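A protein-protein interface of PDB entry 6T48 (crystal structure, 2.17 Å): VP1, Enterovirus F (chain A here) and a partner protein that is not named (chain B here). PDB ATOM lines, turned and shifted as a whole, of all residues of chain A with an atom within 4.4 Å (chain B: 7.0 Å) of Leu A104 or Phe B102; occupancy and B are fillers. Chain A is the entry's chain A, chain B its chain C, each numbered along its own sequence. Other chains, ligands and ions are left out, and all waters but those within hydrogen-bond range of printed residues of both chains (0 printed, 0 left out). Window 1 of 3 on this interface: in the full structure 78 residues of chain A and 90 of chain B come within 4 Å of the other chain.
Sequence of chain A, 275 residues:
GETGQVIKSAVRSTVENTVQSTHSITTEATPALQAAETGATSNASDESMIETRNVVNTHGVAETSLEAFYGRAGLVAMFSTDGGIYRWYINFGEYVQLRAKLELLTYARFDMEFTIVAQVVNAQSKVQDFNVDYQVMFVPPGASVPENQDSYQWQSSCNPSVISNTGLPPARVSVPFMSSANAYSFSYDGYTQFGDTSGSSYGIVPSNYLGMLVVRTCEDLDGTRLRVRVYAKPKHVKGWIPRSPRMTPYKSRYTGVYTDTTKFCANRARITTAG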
ATOM      1  N   PHE A  69      -2.561 -26.151  16.878  1.00  0.00           N
ATOM      2  CA  PHE A  69      -2.206 -24.988  17.681  1.00  0.00           C
ATOM      3  C   PHE A  69      -3.354 -24.561  18.598  1.00  0.00           C
ATOM      4  O   PHE A  69      -3.149 -24.299  19.784  1.00  0.00           O
ATOM      5  CB  PHE A  69      -1.824 -23.825  16.761  1.00  0.00           C
ATOM      6  CG  PHE A  69      -1.303 -22.616  17.487  1.00  0.00           C
ATOM      7  CD1 PHE A  69       0.033 -22.539  17.865  1.00  0.00           C
ATOM      8  CD2 PHE A  69      -2.150 -21.555  17.797  1.00  0.00           C
ATOM      9  CE1 PHE A  69       0.523 -21.419  18.540  1.00  0.00           C
ATOM     10  CE2 PHE A  69      -1.674 -20.431  18.473  1.00  0.00           C
ATOM     11  CZ  PHE A  69      -0.334 -20.363  18.846  1.00  0.00           C
ATOM     12  N   TYR A  70      -4.562 -24.505  18.048  1.00  0.00           N
ATOM     13  CA  TYR A  70      -5.736 -24.072  18.804  1.00  0.00           C
ATOM     14  C   TYR A  70      -6.542 -25.173  19.486  1.00  0.00           C
ATOM     15  O   TYR A  70      -7.251 -24.916  20.458  1.00  0.00           O
ATOM     16  CB  TYR A  70      -6.668 -23.290  17.878  1.00  0.00           C
ATOM     17  CG  TYR A  70      -6.135 -21.939  17.476  1.00  0.00           C
ATOM     18  CD1 TYR A  70      -6.069 -20.897  18.400  1.00  0.00           C
ATOM     19  CD2 TYR A  70      -5.701 -21.697  16.171  1.00  0.00           C
ATOM     20  CE1 TYR A  70      -5.585 -19.642  18.040  1.00  0.00           C
ATOM     21  CE2 TYR A  70      -5.213 -20.443  15.797  1.00  0.00           C
ATOM     22  CZ  TYR A  70      -5.159 -19.422  16.740  1.00  0.00           C
ATOM     23  OH  TYR A  70      -4.676 -18.183  16.396  1.00  0.00           O
ATOM     24  N   ALA A 100      -4.342 -14.030  23.683  1.00  0.00           N
ATOM     25  CA  ALA A 100      -3.186 -13.751  22.837  1.00  0.00           C
ATOM     26  C   ALA A 100      -3.095 -14.718  21.662  1.00  0.00           C
ATOM     27  O   ALA A 100      -2.653 -14.335  20.578  1.00  0.00           O
ATOM     28  CB  ALA A 100      -1.905 -13.806  23.663  1.00  0.00           C
ATOM     29  N   LYS A 101      -3.508 -15.966  21.873  1.00  0.00           N
ATOM     30  CA  LYS A 101      -3.470 -16.967  20.805  1.00  0.00           C
ATOM     31  C   LYS A 101      -4.427 -16.605  19.675  1.00  0.00           C
ATOM     32  O   LYS A 101      -4.057 -16.628  18.503  1.00  0.00           O
ATOM     33  CB  LYS A 101      -3.852 -18.354  21.339  1.00  0.00           C
ATOM     34  CG  LYS A 101      -2.860 -18.961  22.307  1.00  0.00           C
ATOM     35  CD  LYS A 101      -3.291 -20.359  22.747  1.00  0.00           C
ATOM     36  CE  LYS A 101      -3.247 -21.355  21.595  1.00  0.00           C
ATOM     37  NZ  LYS A 101      -3.586 -22.731  22.060  1.00  0.00           N
ATOM     38  N   LEU A 102      -5.663 -16.276  20.032  1.00  0.00           N
ATOM     39  CA  LEU A 102      -6.674 -15.930  19.038  1.00  0.00           C
ATOM     40  C   LEU A 102      -6.305 -14.694  18.230  1.00  0.00           C
ATOM     41  O   LEU A 102      -6.589 -14.620  17.037  1.00  0.00           O
ATOM     42  CB  LEU A 102      -8.025 -15.714  19.722  1.00  0.00           C
ATOM     43  CG  LEU A 102      -8.608 -16.961  20.396  1.00  0.00           C
ATOM     44  CD1 LEU A 102      -9.827 -16.582  21.212  1.00  0.00           C
ATOM     45  CD2 LEU A 102      -8.971 -17.991  19.340  1.00  0.00           C
ATOM     46  N   GLU A 103      -5.668 -13.726  18.877  1.00  0.00           N
ATOM     47  CA  GLU A 103      -5.280 -12.498  18.198  1.00  0.00           C
ATOM     48  C   GLU A 103      -4.154 -12.666  17.173  1.00  0.00           C
ATOM     49  O   GLU A 103      -3.678 -11.686  16.597  1.00  0.00           O
ATOM     50  CB  GLU A 103      -4.936 -11.424  19.235  1.00  0.00           C
ATOM     51  CG  GLU A 103      -6.184 -10.751  19.806  1.00  0.00           C
ATOM     52  CD  GLU A 103      -5.901  -9.824  20.974  1.00  0.00           C
ATOM     53  OE1 GLU A 103      -4.776  -9.281  21.057  1.00  0.00           O
ATOM     54  OE2 GLU A 103      -6.818  -9.625  21.804  1.00  0.00           O
ATOM     55  N   LEU A 104      -3.743 -13.909  16.934  1.00  0.00           N
ATOM     56  CA  LEU A 104      -2.703 -14.200  15.947  1.00  0.00           C
ATOM     57  C   LEU A 104      -3.339 -14.300  14.562  1.00  0.00           C
ATOM     58  O   LEU A 104      -2.647 -14.388  13.546  1.00  0.00           O
ATOM     59  CB  LEU A 104      -2.002 -15.520  16.282  1.00  0.00           C
ATOM     60  CG  LEU A 104      -1.096 -15.501  17.512  1.00  0.00           C
ATOM     61  CD1 LEU A 104      -0.598 -16.911  17.810  1.00  0.00           C
ATOM     62  CD2 LEU A 104       0.070 -14.556  17.260  1.00  0.00           C
ATOM     63  N   LEU A 105      -4.668 -14.299  14.537  1.00  0.00           N
ATOM     64  CA  LEU A 105      -5.435 -14.372  13.298  1.00  0.00           C
ATOM     65  C   LEU A 105      -6.389 -13.184  13.259  1.00  0.00           C
ATOM     66  O   LEU A 105      -6.818 -12.699  14.302  1.00  0.00           O
ATOM     67  CB  LEU A 105      -6.255 -15.664  13.250  1.00  0.00           C
ATOM     68  CG  LEU A 105      -5.490 -16.975  13.076  1.00  0.00           C
ATOM     69  CD1 LEU A 105      -6.436 -18.143  13.256  1.00  0.00           C
ATOM     70  CD2 LEU A 105      -4.851 -17.009  11.703  1.00  0.00           C
ATOM     71  N   PRO A 242      -2.924 -13.700   9.014  1.00  0.00           N
ATOM     72  CA  PRO A 242      -2.085 -13.772  10.216  1.00  0.00           C
ATOM     73  C   PRO A 242      -1.764 -12.357  10.682  1.00  0.00           C
ATOM     74  O   PRO A 242      -1.593 -11.458   9.858  1.00  0.00           O
ATOM     75  CB  PRO A 242      -0.830 -14.491   9.723  1.00  0.00           C
ATOM     76  CG  PRO A 242      -1.310 -15.278   8.552  1.00  0.00           C
ATOM     77  CD  PRO A 242      -2.243 -14.322   7.869  1.00  0.00           C
ATOM     78  N   ARG A 243      -1.668 -12.156  11.991  1.00  0.00           N
ATOM     79  CA  ARG A 243      -1.372 -10.830  12.514  1.00  0.00           C
ATOM     80  C   ARG A 243      -0.063 -10.763  13.289  1.00  0.00           C
ATOM     81  O   ARG A 243       0.503 -11.783  13.676  1.00  0.00           O
ATOM     82  CB  ARG A 243      -2.512 -10.355  13.422  1.00  0.00           C
ATOM     83  CG  ARG A 243      -3.879 -10.342  12.757  1.00  0.00           C
ATOM     84  CD  ARG A 243      -4.872  -9.547  13.587  1.00  0.00           C
ATOM     85  NE  ARG A 243      -4.554  -8.119  13.611  1.00  0.00           N
ATOM     86  CZ  ARG A 243      -4.765  -7.280  12.600  1.00  0.00           C
ATOM     87  NH1 ARG A 243      -5.303  -7.716  11.470  1.00  0.00           N
ATOM     88  NH2 ARG A 243      -4.444  -5.997  12.722  1.00  0.00           N
ATOM     89  N   PRO A 245       2.012 -10.552  16.346  1.00  0.00           N
ATOM     90  CA  PRO A 245       1.738 -10.970  17.732  1.00  0.00           C
ATOM     91  C   PRO A 245       1.750  -9.860  18.785  1.00  0.00           C
ATOM     92  O   PRO A 245       2.481  -8.879  18.658  1.00  0.00           O
ATOM     93  CB  PRO A 245       2.830 -12.004  18.007  1.00  0.00           C
ATOM     94  CG  PRO A 245       3.123 -12.564  16.643  1.00  0.00           C
ATOM     95  CD  PRO A 245       3.130 -11.329  15.781  1.00  0.00           C
ATOM     96  N   VAL B  40      -4.828 -19.137   6.052  1.00  0.00           N
ATOM     97  CA  VAL B  40      -3.620 -19.797   6.521  1.00  0.00           C
ATOM     98  C   VAL B  40      -4.042 -21.134   7.123  1.00  0.00           C
ATOM     99  O   VAL B  40      -5.035 -21.209   7.844  1.00  0.00           O
ATOM    100  CB  VAL B  40      -2.886 -18.930   7.576  1.00  0.00           C
ATOM    101  CG1 VAL B  40      -3.861 -18.450   8.621  1.00  0.00           C
ATOM    102  CG2 VAL B  40      -1.770 -19.728   8.232  1.00  0.00           C
ATOM    103  N   PHE B  43       0.871 -22.536  10.802  1.00  0.00           N
ATOM    104  CA  PHE B  43       1.697 -21.392  11.153  1.00  0.00           C
ATOM    105  C   PHE B  43       3.114 -21.430  10.597  1.00  0.00           C
ATOM    106  O   PHE B  43       3.870 -20.473  10.761  1.00  0.00           O
ATOM    107  CB  PHE B  43       1.699 -21.185  12.668  1.00  0.00           C
ATOM    108  CG  PHE B  43       0.452 -20.517  13.174  1.00  0.00           C
ATOM    109  CD1 PHE B  43       0.108 -19.242  12.731  1.00  0.00           C
ATOM    110  CD2 PHE B  43      -0.393 -21.164  14.069  1.00  0.00           C
ATOM    111  CE1 PHE B  43      -1.062 -18.619  13.172  1.00  0.00           C
ATOM    112  CE2 PHE B  43      -1.567 -20.551  14.516  1.00  0.00           C
ATOM    113  CZ  PHE B  43      -1.901 -19.275  14.065  1.00  0.00           C
ATOM    114  N   LEU B  44       3.480 -22.522   9.934  1.00  0.00           N
ATOM    115  CA  LEU B  44       4.803 -22.589   9.324  1.00  0.00           C
ATOM    116  C   LEU B  44       4.811 -21.580   8.180  1.00  0.00           C
ATOM    117  O   LEU B  44       5.866 -21.108   7.755  1.00  0.00           O
ATOM    118  CB  LEU B  44       5.091 -23.982   8.764  1.00  0.00           C
ATOM    119  CG  LEU B  44       5.534 -25.045   9.763  1.00  0.00           C
ATOM    120  CD1 LEU B  44       5.901 -26.322   9.015  1.00  0.00           C
ATOM    121  CD2 LEU B  44       6.729 -24.527  10.548  1.00  0.00           C
ATOM    122  N   VAL B  46       3.652 -18.672   8.394  1.00  0.00           N
ATOM    123  CA  VAL B  46       3.953 -17.375   8.994  1.00  0.00           C
ATOM    124  C   VAL B  46       5.425 -17.196   9.364  1.00  0.00           C
ATOM    125  O   VAL B  46       6.010 -16.149   9.088  1.00  0.00           O
ATOM    126  CB  VAL B  46       3.089 -17.130  10.254  1.00  0.00           C
ATOM    127  CG1 VAL B  46       3.465 -15.806  10.904  1.00  0.00           C
ATOM    128  CG2 VAL B  46       1.621 -17.124   9.879  1.00  0.00           C
ATOM    129  N   VAL B  47       6.031 -18.205   9.983  1.00  0.00           N
ATOM    130  CA  VAL B  47       7.432 -18.082  10.372  1.00  0.00           C
ATOM    131  C   VAL B  47       8.380 -18.008   9.174  1.00  0.00           C
ATOM    132  O   VAL B  47       9.557 -17.681   9.331  1.00  0.00           O
ATOM    133  CB  VAL B  47       7.871 -19.235  11.312  1.00  0.00           C
ATOM    134  CG1 VAL B  47       7.122 -19.134  12.627  1.00  0.00           C
ATOM    135  CG2 VAL B  47       7.616 -20.579  10.663  1.00  0.00           C
ATOM    136  N   GLN B  95      13.595 -12.657  20.141  1.00  0.00           N
ATOM    137  CA  GLN B  95      12.343 -12.914  20.834  1.00  0.00           C
ATOM    138  C   GLN B  95      11.108 -12.151  20.388  1.00  0.00           C
ATOM    139  O   GLN B  95       9.992 -12.644  20.557  1.00  0.00           O
ATOM    140  CB  GLN B  95      12.533 -12.764  22.347  1.00  0.00           C
ATOM    141  CG  GLN B  95      12.564 -11.349  22.872  1.00  0.00           C
ATOM    142  CD  GLN B  95      12.800 -11.325  24.365  1.00  0.00           C
ATOM    143  OE1 GLN B  95      13.891 -11.633  24.833  1.00  0.00           O
ATOM    144  NE2 GLN B  95      11.772 -10.977  25.123  1.00  0.00           N
ATOM    145  N   THR B  97      10.541 -11.223  17.189  1.00  0.00           N
ATOM    146  CA  THR B  97      10.308 -11.443  15.758  1.00  0.00           C
ATOM    147  C   THR B  97       9.183 -12.462  15.566  1.00  0.00           C
ATOM    148  O   THR B  97       8.786 -13.137  16.518  1.00  0.00           O
ATOM    149  CB  THR B  97      11.570 -11.991  15.050  1.00  0.00           C
ATOM    150  OG1 THR B  97      11.905 -13.273  15.596  1.00  0.00           O
ATOM    151  CG2 THR B  97      12.754 -11.046  15.245  1.00  0.00           C
ATOM    152  N   LEU B  98       8.665 -12.570  14.344  1.00  0.00           N
ATOM    153  CA  LEU B  98       7.601 -13.532  14.059  1.00  0.00           C
ATOM    154  C   LEU B  98       8.119 -14.927  14.356  1.00  0.00           C
ATOM    155  O   LEU B  98       7.468 -15.718  15.039  1.00  0.00           O
ATOM    156  CB  LEU B  98       7.186 -13.470  12.588  1.00  0.00           C
ATOM    157  CG  LEU B  98       6.344 -12.286  12.130  1.00  0.00           C
ATOM    158  CD1 LEU B  98       6.192 -12.332  10.623  1.00  0.00           C
ATOM    159  CD2 LEU B  98       4.987 -12.338  12.808  1.00  0.00           C
ATOM    160  N   LEU B  99       9.299 -15.220  13.823  1.00  0.00           N
ATOM    161  CA  LEU B  99       9.935 -16.511  14.022  1.00  0.00           C
ATOM    162  C   LEU B  99      10.119 -16.767  15.512  1.00  0.00           C
ATOM    163  O   LEU B  99       9.810 -17.849  16.007  1.00  0.00           O
ATOM    164  CB  LEU B  99      11.293 -16.533  13.322  1.00  0.00           C
ATOM    165  CG  LEU B  99      12.153 -17.776  13.541  1.00  0.00           C
ATOM    166  CD1 LEU B  99      11.462 -18.985  12.940  1.00  0.00           C
ATOM    167  CD2 LEU B  99      13.514 -17.573  12.901  1.00  0.00           C
ATOM    168  N   GLY B 100      10.613 -15.760  16.224  1.00  0.00           N
ATOM    169  CA  GLY B 100      10.836 -15.900  17.654  1.00  0.00           C
ATOM    170  C   GLY B 100       9.577 -16.157  18.465  1.00  0.00           C
ATOM    171  O   GLY B 100       9.562 -17.018  19.345  1.00  0.00           O
ATOM    172  N   VAL B 101       8.517 -15.409  18.178  1.00  0.00           N
ATOM    173  CA  VAL B 101       7.264 -15.577  18.904  1.00  0.00           C
ATOM    174  C   VAL B 101       6.737 -17.003  18.792  1.00  0.00           C
ATOM    175  O   VAL B 101       6.459 -17.646  19.801  1.00  0.00           O
ATOM    176  CB  VAL B 101       6.183 -14.602  18.393  1.00  0.00           C
ATOM    177  CG1 VAL B 101       4.825 -14.973  18.977  1.00  0.00           C
ATOM    178  CG2 VAL B 101       6.549 -13.181  18.794  1.00  0.00           C
ATOM    179  N   PHE B 102       6.601 -17.502  17.570  1.00  0.00           N
ATOM    180  CA  PHE B 102       6.101 -18.855  17.385  1.00  0.00           C
ATOM    181  C   PHE B 102       7.057 -19.905  17.921  1.00  0.00           C
ATOM    182  O   PHE B 102       6.628 -20.926  18.453  1.00  0.00           O
ATOM    183  CB  PHE B 102       5.781 -19.098  15.912  1.00  0.00           C
ATOM    184  CG  PHE B 102       4.463 -18.514  15.493  1.00  0.00           C
ATOM    185  CD1 PHE B 102       3.271 -19.159  15.819  1.00  0.00           C
ATOM    186  CD2 PHE B 102       4.405 -17.291  14.834  1.00  0.00           C
ATOM    187  CE1 PHE B 102       2.041 -18.592  15.498  1.00  0.00           C
ATOM    188  CE2 PHE B 102       3.178 -16.713  14.508  1.00  0.00           C
ATOM    189  CZ  PHE B 102       1.994 -17.365  14.841  1.00  0.00           C
ATOM    190  N   THR B 103       8.356 -19.661  17.797  1.00  0.00           N
ATOM    191  CA  THR B 103       9.313 -20.616  18.325  1.00  0.00           C
ATOM    192  C   THR B 103       9.120 -20.676  19.838  1.00  0.00           C
ATOM    193  O   THR B 103       9.268 -21.732  20.447  1.00  0.00           O
ATOM    194  CB  THR B 103      10.762 -20.206  18.007  1.00  0.00           C
ATOM    195  OG1 THR B 103      10.962 -20.229  16.588  1.00  0.00           O
ATOM    196  CG2 THR B 103      11.739 -21.173  18.654  1.00  0.00           C
ATOM    197  N   ARG B 104       8.765 -19.543  20.440  1.00  0.00           N
ATOM    198  CA  ARG B 104       8.548 -19.491  21.880  1.00  0.00           C
ATOM    199  C   ARG B 104       7.228 -20.146  22.308  1.00  0.00           C
ATOM    200  O   ARG B 104       6.961 -20.297  23.500  1.00  0.00           O
ATOM    201  CB  ARG B 104       8.653 -18.040  22.372  1.00  0.00           C
ATOM    202  CG  ARG B 104      10.099 -17.529  22.348  1.00  0.00           C
ATOM    203  CD  ARG B 104      10.191 -16.011  22.381  1.00  0.00           C
ATOM    204  NE  ARG B 104      10.062 -15.441  23.721  1.00  0.00           N
ATOM    205  CZ  ARG B 104      11.019 -15.470  24.646  1.00  0.00           C
ATOM    206  NH1 ARG B 104      12.185 -16.046  24.389  1.00  0.00           N
ATOM    207  NH2 ARG B 104      10.816 -14.896  25.825  1.00  0.00           N
ATOM    208  N   TYR B 105       6.411 -20.543  21.334  1.00  0.00           N
ATOM    209  CA  TYR B 105       5.158 -21.247  21.622  1.00  0.00           C
ATOM    210  C   TYR B 105       5.432 -22.755  21.578  1.00  0.00           C
ATOM    211  O   TYR B 105       4.531 -23.565  21.801  1.00  0.00           O
ATOM    212  CB  TYR B 105       4.075 -20.918  20.584  1.00  0.00           C
ATOM    213  CG  TYR B 105       3.090 -19.846  21.006  1.00  0.00           C
ATOM    214  CD1 TYR B 105       2.209 -20.055  22.069  1.00  0.00           C
ATOM    215  CD2 TYR B 105       3.031 -18.629  20.333  1.00  0.00           C
ATOM    216  CE1 TYR B 105       1.289 -19.071  22.449  1.00  0.00           C
ATOM    217  CE2 TYR B 105       2.118 -17.640  20.703  1.00  0.00           C
ATOM    218  CZ  TYR B 105       1.252 -17.866  21.758  1.00  0.00           C
ATOM    219  OH  TYR B 105       0.354 -16.885  22.115  1.00  0.00           O
ATOM    220  N   TYR B 106       6.676 -23.126  21.277  1.00  0.00           N
ATOM    221  CA  TYR B 106       7.057 -24.537  21.197  1.00  0.00           C
ATOM    222  C   TYR B 106       8.325 -24.864  21.973  1.00  0.00           C
ATOM    223  O   TYR B 106       9.105 -23.976  22.307  1.00  0.00           O
ATOM    224  CB  TYR B 106       7.230 -24.960  19.738  1.00  0.00           C
ATOM    225  CG  TYR B 106       5.928 -24.984  18.976  1.00  0.00           C
ATOM    226  CD1 TYR B 106       5.388 -23.812  18.442  1.00  0.00           C
ATOM    227  CD2 TYR B 106       5.211 -26.170  18.825  1.00  0.00           C
ATOM    228  CE1 TYR B 106       4.160 -23.821  17.776  1.00  0.00           C
ATOM    229  CE2 TYR B 106       3.977 -26.193  18.163  1.00  0.00           C
ATOM    230  CZ  TYR B 106       3.460 -25.015  17.643  1.00  0.00           C
ATOM    231  OH  TYR B 106       2.242 -25.028  17.003  1.00  0.00           O
ATOM    232  N   ALA B 107       8.534 -26.148  22.245  1.00  0.00           N
ATOM    233  CA  ALA B 107       9.698 -26.579  23.006  1.00  0.00           C
ATOM    234  C   ALA B 107      10.891 -27.027  22.163  1.00  0.00           C
ATOM    235  O   ALA B 107      12.021 -27.014  22.644  1.00  0.00           O
ATOM    236  CB  ALA B 107       9.297 -27.698  23.968  1.00  0.00           C
ATOM    237  N   THR B 178      14.192 -25.215  22.368  1.00  0.00           N
ATOM    238  CA  THR B 178      14.078 -23.798  22.028  1.00  0.00           C
ATOM    239  C   THR B 178      14.632 -22.858  23.092  1.00  0.00           C
ATOM    240  O   THR B 178      14.750 -21.657  22.863  1.00  0.00           O
ATOM    241  CB  THR B 178      12.623 -23.415  21.738  1.00  0.00           C
ATOM    242  OG1 THR B 178      11.808 -23.766  22.862  1.00  0.00           O
ATOM    243  CG2 THR B 178      12.126 -24.148  20.498  1.00  0.00           C
ATOM    244  N   PHE B 225      12.109 -26.115   7.945  1.00  0.00           N
ATOM    245  CA  PHE B 225      11.915 -25.772   9.350  1.00  0.00           C
ATOM    246  C   PHE B 225      10.599 -26.290   9.949  1.00  0.00           C
ATOM    247  O   PHE B 225       9.566 -26.292   9.287  1.00  0.00           O
ATOM    248  CB  PHE B 225      11.999 -24.245   9.466  1.00  0.00           C
ATOM    249  CG  PHE B 225      11.838 -23.708  10.859  1.00  0.00           C
ATOM    250  CD1 PHE B 225      10.575 -23.553  11.420  1.00  0.00           C
ATOM    251  CD2 PHE B 225      12.950 -23.292  11.584  1.00  0.00           C
ATOM    252  CE1 PHE B 225      10.418 -22.983  12.680  1.00  0.00           C
ATOM    253  CE2 PHE B 225      12.806 -22.722  12.847  1.00  0.00           C
ATOM    254  CZ  PHE B 225      11.535 -22.566  13.396  1.00  0.00           C
ATOM    255  N   LEU B 227       8.454 -27.128  14.104  1.00  0.00           N
ATOM    256  CA  LEU B 227       8.416 -26.972  15.557  1.00  0.00           C
ATOM    257  C   LEU B 227       7.624 -28.109  16.194  1.00  0.00           C
ATOM    258  O   LEU B 227       6.724 -28.658  15.568  1.00  0.00           O
ATOM    259  CB  LEU B 227       7.754 -25.638  15.911  1.00  0.00           C
ATOM    260  CG  LEU B 227       8.464 -24.384  15.405  1.00  0.00           C
ATOM    261  CD1 LEU B 227       7.535 -23.183  15.510  1.00  0.00           C
ATOM    262  CD2 LEU B 227       9.732 -24.166  16.218  1.00  0.00           C
ATOM    263  N   LEU B 230       3.845 -27.927  21.805  1.00  0.00           N
ATOM    264  CA  LEU B 230       3.298 -26.617  22.119  1.00  0.00           C
ATOM    265  C   LEU B 230       3.466 -26.309  23.606  1.00  0.00           C
ATOM    266  O   LEU B 230       3.357 -27.197  24.451  1.00  0.00           O
ATOM    267  CB  LEU B 230       1.813 -26.577  21.750  1.00  0.00           C
ATOM    268  CG  LEU B 230       1.126 -25.211  21.813  1.00  0.00           C
ATOM    269  CD1 LEU B 230       1.627 -24.351  20.669  1.00  0.00           C
ATOM    270  CD2 LEU B 230      -0.381 -25.382  21.716  1.00  0.00           C
ATOM    271  N   LYS B 231       3.737 -25.048  23.922  1.00  0.00           N
ATOM    272  CA  LYS B 231       3.898 -24.622  25.307  1.00  0.00           C
ATOM    273  C   LYS B 231       3.465 -23.165  25.382  1.00  0.00           C
ATOM    274  O   LYS B 231       3.448 -22.467  24.371  1.00  0.00           O
ATOM    275  CB  LYS B 231       5.360 -24.765  25.756  1.00  0.00           C
ATOM    276  CG  LYS B 231       6.322 -23.696  25.230  1.00  0.00           C
ATOM    277  CD  LYS B 231       7.751 -24.015  25.656  1.00  0.00           C
ATOM    278  CE  LYS B 231       8.631 -22.770  25.728  1.00  0.00           C
ATOM    279  NZ  LYS B 231       8.861 -22.136  24.410  1.00  0.00           N
ATOM    280  N   ARG B 233       3.551 -19.299  25.713  1.00  0.00           N
ATOM    281  CA  ARG B 233       4.530 -18.264  25.416  1.00  0.00           C
ATOM    282  C   ARG B 233       4.835 -17.522  26.720  1.00  0.00           C
ATOM    283  O   ARG B 233       3.957 -16.895  27.309  1.00  0.00           O
ATOM    284  CB  ARG B 233       3.949 -17.320  24.365  1.00  0.00           C
ATOM    285  CG  ARG B 233       4.885 -16.239  23.911  1.00  0.00           C
ATOM    286  CD  ARG B 233       4.176 -15.291  22.970  1.00  0.00           C
ATOM    287  NE  ARG B 233       4.940 -14.060  22.817  1.00  0.00           N
ATOM    288  CZ  ARG B 233       4.447 -12.934  22.318  1.00  0.00           C
ATOM    289  NH1 ARG B 233       3.183 -12.883  21.916  1.00  0.00           N
ATOM    290  NH2 ARG B 233       5.214 -11.854  22.245  1.00  0.00           N
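O of Phe A69 sits at hydrogen-bond distance from NZ of Lys A101, at 2.8 Å. The backbone carbonyl oxygen of Lys A101 is in hydrogen-bond range of the side-chain hydroxyl of Tyr A70 (2.7 Å). O of Leu A104 lies within hydrogen-bond range of N of Arg A243 (2.9 Å). O of Tyr B105 is in hydrogen-bond range of N of Lys B231 (2.7 Å). The backbone carbonyl oxygen (O) of Tyr B106 sits at hydrogen-bond distance from the side-chain hydroxyl (OG1) of Thr B178 (2.8 Å). O of Tyr B106 is in hydrogen-bond range of NZ of Lys B231 (2.8 Å).
Among the printed residues, pairs that only touch across the chains: Phe A69 with Phe B43 (3.5 Å), Phe A69 with Tyr B105 (3.9 Å), Phe A69 with Tyr B106 (3.4 Å), Phe A69 with Leu B230 (3.5 Å), Tyr A70 with Phe B43 (3.8 Å), Lys A101 with Tyr B105 (3.8 Å), Leu A104 with Phe B102 (3.9 Å), Leu A105 with Val B40 (3.5 Å), Pro A242 with Val B46 (3.6 Å), Pro A245 with Leu B98 (3.6 Å) and Pro A245 with Val B101 (3.7 Å).
Leu A104 touches just one residue of chain B: Phe B102. Phe B102 touches one residue of chain A. Printed residues of chain B within 4 Å of Phe A69: Phe B43, Tyr B105, Tyr B106 and Leu B230. Of the printed residues of chain A, Tyr B106 touches Phe A69 (3.4 Å). Leu B44 touches none of the printed residues of chain A. Lys B231 touches none of the printed residues of chain A. The nearest printed residue of chain A that does not touch Phe B102 is Phe A69 (4.4 Å).
Of the 11 printed residues of chain A, 7 touch a printed residue of chain B. Hydrophobic or aromatic side chains of chain A within 4 Å of the printed part of chain B: Phe A69, Tyr A70, Leu A104, Leu A105, Pro A242 and Pro A245. Of the 23 printed residues of chain B, 9 touch a printed residue of chain A. Printed residues of chain B that touch a printed residue of chain A: Val B40, Phe B43, Val B46, Leu B98, Val B101, Phe B102, Tyr B105, Tyr B106 and Leu B230.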
